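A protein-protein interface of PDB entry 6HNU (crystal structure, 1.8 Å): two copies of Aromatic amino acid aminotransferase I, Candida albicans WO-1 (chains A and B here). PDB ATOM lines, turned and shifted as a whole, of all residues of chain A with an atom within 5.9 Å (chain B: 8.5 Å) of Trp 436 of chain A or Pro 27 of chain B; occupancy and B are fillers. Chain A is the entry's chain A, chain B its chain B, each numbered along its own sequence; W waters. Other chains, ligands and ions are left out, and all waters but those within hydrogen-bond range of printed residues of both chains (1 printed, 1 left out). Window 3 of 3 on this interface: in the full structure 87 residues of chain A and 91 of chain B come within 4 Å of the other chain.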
ATOM      1  N   THR A 165      19.643 -34.120  -9.741  1.00  0.00           N
ATOM      2  CA  THR A 165      21.126 -34.099  -9.855  1.00  0.00           C
ATOM      3  C   THR A 165      21.711 -32.958  -9.011  1.00  0.00           C
ATOM      4  O   THR A 165      21.002 -32.330  -8.227  1.00  0.00           O
ATOM      5  CB  THR A 165      21.535 -34.068 -11.330  1.00  0.00           C
ATOM      6  OG1 THR A 165      22.949 -34.288 -11.410  1.00  0.00           O
ATOM      7  CG2 THR A 165      21.155 -32.768 -12.003  1.00  0.00           C
ATOM      8  N   SER A 167      23.153 -29.667  -7.660  1.00  0.00           N
ATOM      9  CA  SER A 167      22.768 -28.245  -7.847  1.00  0.00           C
ATOM     10  C   SER A 167      23.929 -27.425  -8.425  1.00  0.00           C
ATOM     11  O   SER A 167      23.663 -26.669  -9.334  1.00  0.00           O
ATOM     12  CB  SER A 167      22.327 -27.649  -6.560  1.00  0.00           C
ATOM     13  OG  SER A 167      23.465 -27.447  -5.735  1.00  0.00           O
ATOM     14  N   GLU A 417       5.666 -32.574   0.913  1.00  0.00           N
ATOM     15  CA  GLU A 417       7.141 -32.487   1.129  1.00  0.00           C
ATOM     16  C   GLU A 417       7.470 -31.362   2.124  1.00  0.00           C
ATOM     17  O   GLU A 417       8.245 -31.603   3.101  1.00  0.00           O
ATOM     18  CB  GLU A 417       7.861 -32.279  -0.192  1.00  0.00           C
ATOM     19  CG  GLU A 417       9.372 -32.413  -0.103  1.00  0.00           C
ATOM     20  CD  GLU A 417      10.037 -31.960  -1.381  1.00  0.00           C
ATOM     21  OE1 GLU A 417       9.742 -30.822  -1.849  1.00  0.00           O
ATOM     22  OE2 GLU A 417      10.821 -32.746  -1.938  1.00  0.00           O
ATOM     23  N   HIS A 421       9.044 -31.756   5.809  1.00  0.00           N
ATOM     24  CA  HIS A 421      10.318 -31.008   6.048  1.00  0.00           C
ATOM     25  C   HIS A 421      10.180 -30.172   7.334  1.00  0.00           C
ATOM     26  O   HIS A 421      11.006 -30.321   8.250  1.00  0.00           O
ATOM     27  CB  HIS A 421      10.698 -30.194   4.809  1.00  0.00           C
ATOM     28  CG  HIS A 421      12.018 -29.527   4.884  1.00  0.00           C
ATOM     29  ND1 HIS A 421      13.176 -30.232   5.147  1.00  0.00           N
ATOM     30  CD2 HIS A 421      12.359 -28.231   4.758  1.00  0.00           C
ATOM     31  CE1 HIS A 421      14.182 -29.376   5.144  1.00  0.00           C
ATOM     32  NE2 HIS A 421      13.707 -28.141   4.944  1.00  0.00           N
ATOM     33  N   ALA A 432      17.402 -33.116   3.244  1.00  0.00           N
ATOM     34  CA  ALA A 432      17.222 -32.210   2.102  1.00  0.00           C
ATOM     35  C   ALA A 432      16.018 -32.661   1.286  1.00  0.00           C
ATOM     36  O   ALA A 432      15.978 -33.799   0.807  1.00  0.00           O
ATOM     37  CB  ALA A 432      18.481 -32.237   1.256  1.00  0.00           C
ATOM     38  N   PRO A 433      15.018 -31.793   1.039  1.00  0.00           N
ATOM     39  CA  PRO A 433      13.923 -32.154   0.144  1.00  0.00           C
ATOM     40  C   PRO A 433      14.391 -32.534  -1.263  1.00  0.00           C
ATOM     41  O   PRO A 433      15.134 -31.795  -1.888  1.00  0.00           O
ATOM     42  CB  PRO A 433      13.032 -30.892   0.176  1.00  0.00           C
ATOM     43  CG  PRO A 433      13.317 -30.277   1.498  1.00  0.00           C
ATOM     44  CD  PRO A 433      14.793 -30.516   1.732  1.00  0.00           C
ATOM     45  N   GLY A 434      13.873 -33.664  -1.759  1.00  0.00           N
ATOM     46  CA  GLY A 434      14.199 -34.214  -3.086  1.00  0.00           C
ATOM     47  C   GLY A 434      13.908 -33.229  -4.216  1.00  0.00           C
ATOM     48  O   GLY A 434      14.702 -33.162  -5.167  1.00  0.00           O
ATOM     49  N   SER A 435      12.809 -32.463  -4.115  1.00  0.00           N
ATOM     50  CA  SER A 435      12.357 -31.544  -5.190  1.00  0.00           C
ATOM     51  C   SER A 435      13.420 -30.457  -5.425  1.00  0.00           C
ATOM     52  O   SER A 435      13.505 -29.981  -6.515  1.00  0.00           O
ATOM     53  CB  SER A 435      11.014 -30.928  -4.872  1.00  0.00           C
ATOM     54  OG  SER A 435      11.141 -29.998  -3.809  1.00  0.00           O
ATOM     55  N   TRP A 436      14.254 -30.145  -4.448  1.00  0.00           N
ATOM     56  CA  TRP A 436      15.285 -29.078  -4.589  1.00  0.00           C
ATOM     57  C   TRP A 436      16.308 -29.509  -5.628  1.00  0.00           C
ATOM     58  O   TRP A 436      16.978 -28.621  -6.173  1.00  0.00           O
ATOM     59  CB  TRP A 436      15.927 -28.757  -3.253  1.00  0.00           C
ATOM     60  CG  TRP A 436      15.006 -28.155  -2.242  1.00  0.00           C
ATOM     61  CD1 TRP A 436      13.659 -27.958  -2.335  1.00  0.00           C
ATOM     62  CD2 TRP A 436      15.383 -27.713  -0.933  1.00  0.00           C
ATOM     63  NE1 TRP A 436      13.177 -27.402  -1.174  1.00  0.00           N
ATOM     64  CE2 TRP A 436      14.212 -27.249  -0.296  1.00  0.00           C
ATOM     65  CE3 TRP A 436      16.597 -27.665  -0.243  1.00  0.00           C
ATOM     66  CZ2 TRP A 436      14.238 -26.721   0.990  1.00  0.00           C
ATOM     67  CZ3 TRP A 436      16.618 -27.152   1.036  1.00  0.00           C
ATOM     68  CH2 TRP A 436      15.450 -26.689   1.639  1.00  0.00           C
ATOM     69  N   PHE A 437      16.396 -30.815  -5.948  1.00  0.00           N
ATOM     70  CA  PHE A 437      17.446 -31.364  -6.860  1.00  0.00           C
ATOM     71  C   PHE A 437      16.921 -31.596  -8.268  1.00  0.00           C
ATOM     72  O   PHE A 437      17.666 -32.043  -9.138  1.00  0.00           O
ATOM     73  CB  PHE A 437      17.989 -32.698  -6.347  1.00  0.00           C
ATOM     74  CG  PHE A 437      18.621 -32.599  -4.981  1.00  0.00           C
ATOM     75  CD1 PHE A 437      19.949 -32.248  -4.835  1.00  0.00           C
ATOM     76  CD2 PHE A 437      17.869 -32.821  -3.841  1.00  0.00           C
ATOM     77  CE1 PHE A 437      20.520 -32.149  -3.578  1.00  0.00           C
ATOM     78  CE2 PHE A 437      18.426 -32.700  -2.580  1.00  0.00           C
ATOM     79  CZ  PHE A 437      19.759 -32.362  -2.455  1.00  0.00           C
ATOM     80  N   LYS A 438      15.651 -31.313  -8.489  1.00  0.00           N
ATOM     81  CA  LYS A 438      15.037 -31.517  -9.823  1.00  0.00           C
ATOM     82  C   LYS A 438      15.707 -30.611 -10.870  1.00  0.00           C
ATOM     83  O   LYS A 438      15.820 -29.381 -10.649  1.00  0.00           O
ATOM     84  CB  LYS A 438      13.537 -31.246  -9.721  1.00  0.00           C
ATOM     85  CG  LYS A 438      12.772 -31.556 -10.986  1.00  0.00           C
ATOM     86  CD  LYS A 438      12.693 -33.044 -11.295  1.00  0.00           C
ATOM     87  CE  LYS A 438      11.888 -33.324 -12.549  1.00  0.00           C
ATOM     88  NZ  LYS A 438      12.697 -33.087 -13.772  1.00  0.00           N
ATOM     89  N   GLN B  24      23.265 -17.666  -9.234  1.00  0.00           N
ATOM     90  CA  GLN B  24      22.505 -17.824  -7.958  1.00  0.00           C
ATOM     91  C   GLN B  24      23.325 -18.609  -6.942  1.00  0.00           C
ATOM     92  O   GLN B  24      24.273 -19.287  -7.337  1.00  0.00           O
ATOM     93  CB  GLN B  24      21.180 -18.535  -8.208  1.00  0.00           C
ATOM     94  CG  GLN B  24      20.398 -17.964  -9.375  1.00  0.00           C
ATOM     95  CD  GLN B  24      19.002 -18.533  -9.448  1.00  0.00           C
ATOM     96  OE1 GLN B  24      18.251 -18.508  -8.474  1.00  0.00           O
ATOM     97  NE2 GLN B  24      18.647 -19.067 -10.604  1.00  0.00           N
ATOM     98  N   THR B  25      22.978 -18.498  -5.655  1.00  0.00           N
ATOM     99  CA  THR B  25      23.495 -19.387  -4.583  1.00  0.00           C
ATOM    100  C   THR B  25      22.799 -20.746  -4.715  1.00  0.00           C
ATOM    101  O   THR B  25      21.726 -20.800  -5.376  1.00  0.00           O
ATOM    102  CB  THR B  25      23.273 -18.820  -3.177  1.00  0.00           C
ATOM    103  OG1 THR B  25      21.890 -18.461  -3.093  1.00  0.00           O
ATOM    104  CG2 THR B  25      24.160 -17.632  -2.881  1.00  0.00           C
ATOM    105  N   SER B  26      23.403 -21.787  -4.133  1.00  0.00           N
ATOM    106  CA  SER B  26      22.852 -23.165  -4.018  1.00  0.00           C
ATOM    107  C   SER B  26      21.426 -23.114  -3.455  1.00  0.00           C
ATOM    108  O   SER B  26      21.147 -22.329  -2.551  1.00  0.00           O
ATOM    109  CB  SER B  26      23.764 -24.012  -3.154  1.00  0.00           C
ATOM    110  OG  SER B  26      23.557 -25.395  -3.390  1.00  0.00           O
ATOM    111  N   PRO B  27      20.460 -23.918  -3.967  1.00  0.00           N
ATOM    112  CA  PRO B  27      19.174 -24.089  -3.286  1.00  0.00           C
ATOM    113  C   PRO B  27      19.302 -24.718  -1.885  1.00  0.00           C
ATOM    114  O   PRO B  27      18.327 -24.683  -1.170  1.00  0.00           O
ATOM    115  CB  PRO B  27      18.346 -24.993  -4.217  1.00  0.00           C
ATOM    116  CG  PRO B  27      19.360 -25.632  -5.155  1.00  0.00           C
ATOM    117  CD  PRO B  27      20.529 -24.666  -5.230  1.00  0.00           C
ATOM    118  N   LEU B  28      20.488 -25.237  -1.522  1.00  0.00           N
ATOM    119  CA  LEU B  28      20.806 -25.806  -0.181  1.00  0.00           C
ATOM    120  C   LEU B  28      21.415 -24.731   0.738  1.00  0.00           C
ATOM    121  O   LEU B  28      21.897 -25.091   1.836  1.00  0.00           O
ATOM    122  CB  LEU B  28      21.780 -26.980  -0.339  1.00  0.00           C
ATOM    123  CG  LEU B  28      21.392 -28.090  -1.323  1.00  0.00           C
ATOM    124  CD1 LEU B  28      22.108 -29.371  -0.960  1.00  0.00           C
ATOM    125  CD2 LEU B  28      19.895 -28.339  -1.368  1.00  0.00           C
ATOM    126  N   LYS B  29      21.417 -23.460   0.328  1.00  0.00           N
ATOM    127  CA  LYS B  29      21.691 -22.319   1.246  1.00  0.00           C
ATOM    128  C   LYS B  29      20.531 -22.248   2.251  1.00  0.00           C
ATOM    129  O   LYS B  29      20.791 -21.971   3.438  1.00  0.00           O
ATOM    130  CB  LYS B  29      21.871 -21.010   0.464  1.00  0.00           C
ATOM    131  N   GLY B  30      19.315 -22.579   1.790  1.00  0.00           N
ATOM    132  CA  GLY B  30      18.044 -22.516   2.539  1.00  0.00           C
ATOM    133  C   GLY B  30      17.934 -23.500   3.703  1.00  0.00           C
ATOM    134  O   GLY B  30      16.861 -23.479   4.350  1.00  0.00           O
ATOM    135  N   ILE B  31      18.949 -24.343   3.964  1.00  0.00           N
ATOM    136  CA  ILE B  31      19.023 -25.184   5.201  1.00  0.00           C
ATOM    137  C   ILE B  31      20.322 -24.909   5.966  1.00  0.00           C
ATOM    138  O   ILE B  31      20.485 -25.497   7.038  1.00  0.00           O
ATOM    139  CB  ILE B  31      18.869 -26.695   4.916  1.00  0.00           C
ATOM    140  CG1 ILE B  31      19.906 -27.221   3.917  1.00  0.00           C
ATOM    141  CG2 ILE B  31      17.440 -27.009   4.502  1.00  0.00           C
ATOM    142  CD1 ILE B  31      19.877 -28.725   3.733  1.00  0.00           C
ATOM    143  N   PHE B  32      21.222 -24.075   5.452  1.00  0.00           N
ATOM    144  CA  PHE B  32      22.557 -23.874   6.076  1.00  0.00           C
ATOM    145  C   PHE B  32      22.401 -23.401   7.532  1.00  0.00           C
ATOM    146  O   PHE B  32      23.186 -23.838   8.388  1.00  0.00           O
ATOM    147  CB  PHE B  32      23.423 -22.899   5.269  1.00  0.00           C
ATOM    148  CG  PHE B  32      24.801 -22.709   5.857  1.00  0.00           C
ATOM    149  CD1 PHE B  32      25.754 -23.718   5.779  1.00  0.00           C
ATOM    150  CD2 PHE B  32      25.131 -21.542   6.536  1.00  0.00           C
ATOM    151  CE1 PHE B  32      27.012 -23.553   6.340  1.00  0.00           C
ATOM    152  CE2 PHE B  32      26.389 -21.379   7.098  1.00  0.00           C
ATOM    153  CZ  PHE B  32      27.326 -22.386   7.000  1.00  0.00           C
ATOM    154  N   TYR B  34      20.628 -24.113   9.903  1.00  0.00           N
ATOM    155  CA  TYR B  34      20.378 -25.223  10.864  1.00  0.00           C
ATOM    156  C   TYR B  34      21.660 -26.036  11.105  1.00  0.00           C
ATOM    157  O   TYR B  34      21.651 -26.937  11.984  1.00  0.00           O
ATOM    158  CB  TYR B  34      19.306 -26.171  10.325  1.00  0.00           C
ATOM    159  CG  TYR B  34      17.947 -25.561  10.088  1.00  0.00           C
ATOM    160  CD1 TYR B  34      17.154 -25.181  11.154  1.00  0.00           C
ATOM    161  CD2 TYR B  34      17.435 -25.398   8.808  1.00  0.00           C
ATOM    162  CE1 TYR B  34      15.900 -24.628  10.957  1.00  0.00           C
ATOM    163  CE2 TYR B  34      16.179 -24.854   8.592  1.00  0.00           C
ATOM    164  CZ  TYR B  34      15.410 -24.468   9.677  1.00  0.00           C
ATOM    165  OH  TYR B  34      14.176 -23.923   9.509  1.00  0.00           O
ATOM    166  N   PHE B  42      21.649 -32.718  11.809  1.00  0.00           N
ATOM    167  CA  PHE B  42      21.735 -32.160  10.446  1.00  0.00           C
ATOM    168  C   PHE B  42      22.196 -33.248   9.461  1.00  0.00           C
ATOM    169  O   PHE B  42      23.417 -33.512   9.403  1.00  0.00           O
ATOM    170  CB  PHE B  42      22.671 -30.947  10.401  1.00  0.00           C
ATOM    171  CG  PHE B  42      22.592 -30.225   9.081  1.00  0.00           C
ATOM    172  CD1 PHE B  42      21.627 -29.252   8.873  1.00  0.00           C
ATOM    173  CD2 PHE B  42      23.450 -30.538   8.036  1.00  0.00           C
ATOM    174  CE1 PHE B  42      21.546 -28.583   7.658  1.00  0.00           C
ATOM    175  CE2 PHE B  42      23.348 -29.887   6.816  1.00  0.00           C
ATOM    176  CZ  PHE B  42      22.394 -28.917   6.628  1.00  0.00           C
ATOM    177  N   GLY B  44      21.186 -33.131   6.082  1.00  0.00           N
ATOM    178  CA  GLY B  44      20.802 -32.539   4.777  1.00  0.00           C
ATOM    179  C   GLY B  44      22.010 -32.135   3.939  1.00  0.00           C
ATOM    180  O   GLY B  44      21.809 -31.678   2.791  1.00  0.00           O
HETATM  181  O   HOH W   1      14.431 -25.229   4.892  1.00  0.00           O
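OG of Ser 167 of chain A is in hydrogen-bond range of OG of Ser 26 of chain B.
CB of Ser 167 of chain A touches CD of Pro 27 of chain B, 3.7 Å away.
Ile 31 of chain B touches His 421 of chain A.
CB of Ala 432 of chain A touches O of Gly 44 of chain B, at 3.7 Å.
Pro 27 of chain B touches Trp 436 of chain A (O to CE3, 3.6 Å).
Trp 436 of chain A touches Leu 28 of chain B.
Trp 436 of chain A touches Ile 31 of chain B.
Printed residues of chain B within 4 Å of Ser 167 of chain A: Ser 26 and Pro 27.
Printed residues of chain B within 4 Å of Ala 432 of chain A: Gly 44 (3.7 Å).
No residue of chain B comes within 4 Å of Ser 435 of chain A.
Trp 436 of chain A touches just these residues of chain B: Pro 27 (3.6 Å), Leu 28 (3.5 Å) and Ile 31 (3.5 Å).
Phe 437 of chain A touches none of the printed residues of chain B.
Of the printed residues of chain A, Ser 26 of chain B touches Ser 167 (3.1 Å).
Printed residues of chain A within 4 Å of Pro 27 of chain B: Ser 167 and Trp 436.
Of the printed residues of chain A, Leu 28 of chain B touches Trp 436 (3.5 Å).
Phe 42 of chain B touches none of the printed residues of chain A.
The nearest residue of chain B that does not touch Trp 436 of chain A is Gly 30 of chain B (4.4 Å).
The nearest printed residue of chain A that does not touch Gly 44 of chain B is Phe 437 of chain A (5.7 Å).
Of the 11 printed residues of chain A, 4 touch a printed residue of chain B.
Printed residues of chain A that touch a printed residue of chain B: Ser 167, His 421, Ala 432 and Trp 436.
Hydrophobic or aromatic side chains of chain A within 4 Å of the printed part of chain B: His 421, Ala 432 and Trp 436.
Hydrophobic or aromatic side chains of chain B that line the printed part of chain A: Pro 27, Leu 28 and Ile 31.
No position is printed for both chains.
Water W1 lies within hydrogen-bond range of NE2 of His 421 of chain A (3.0 Å) and O of Gly 30 of chain B (3.0 Å).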
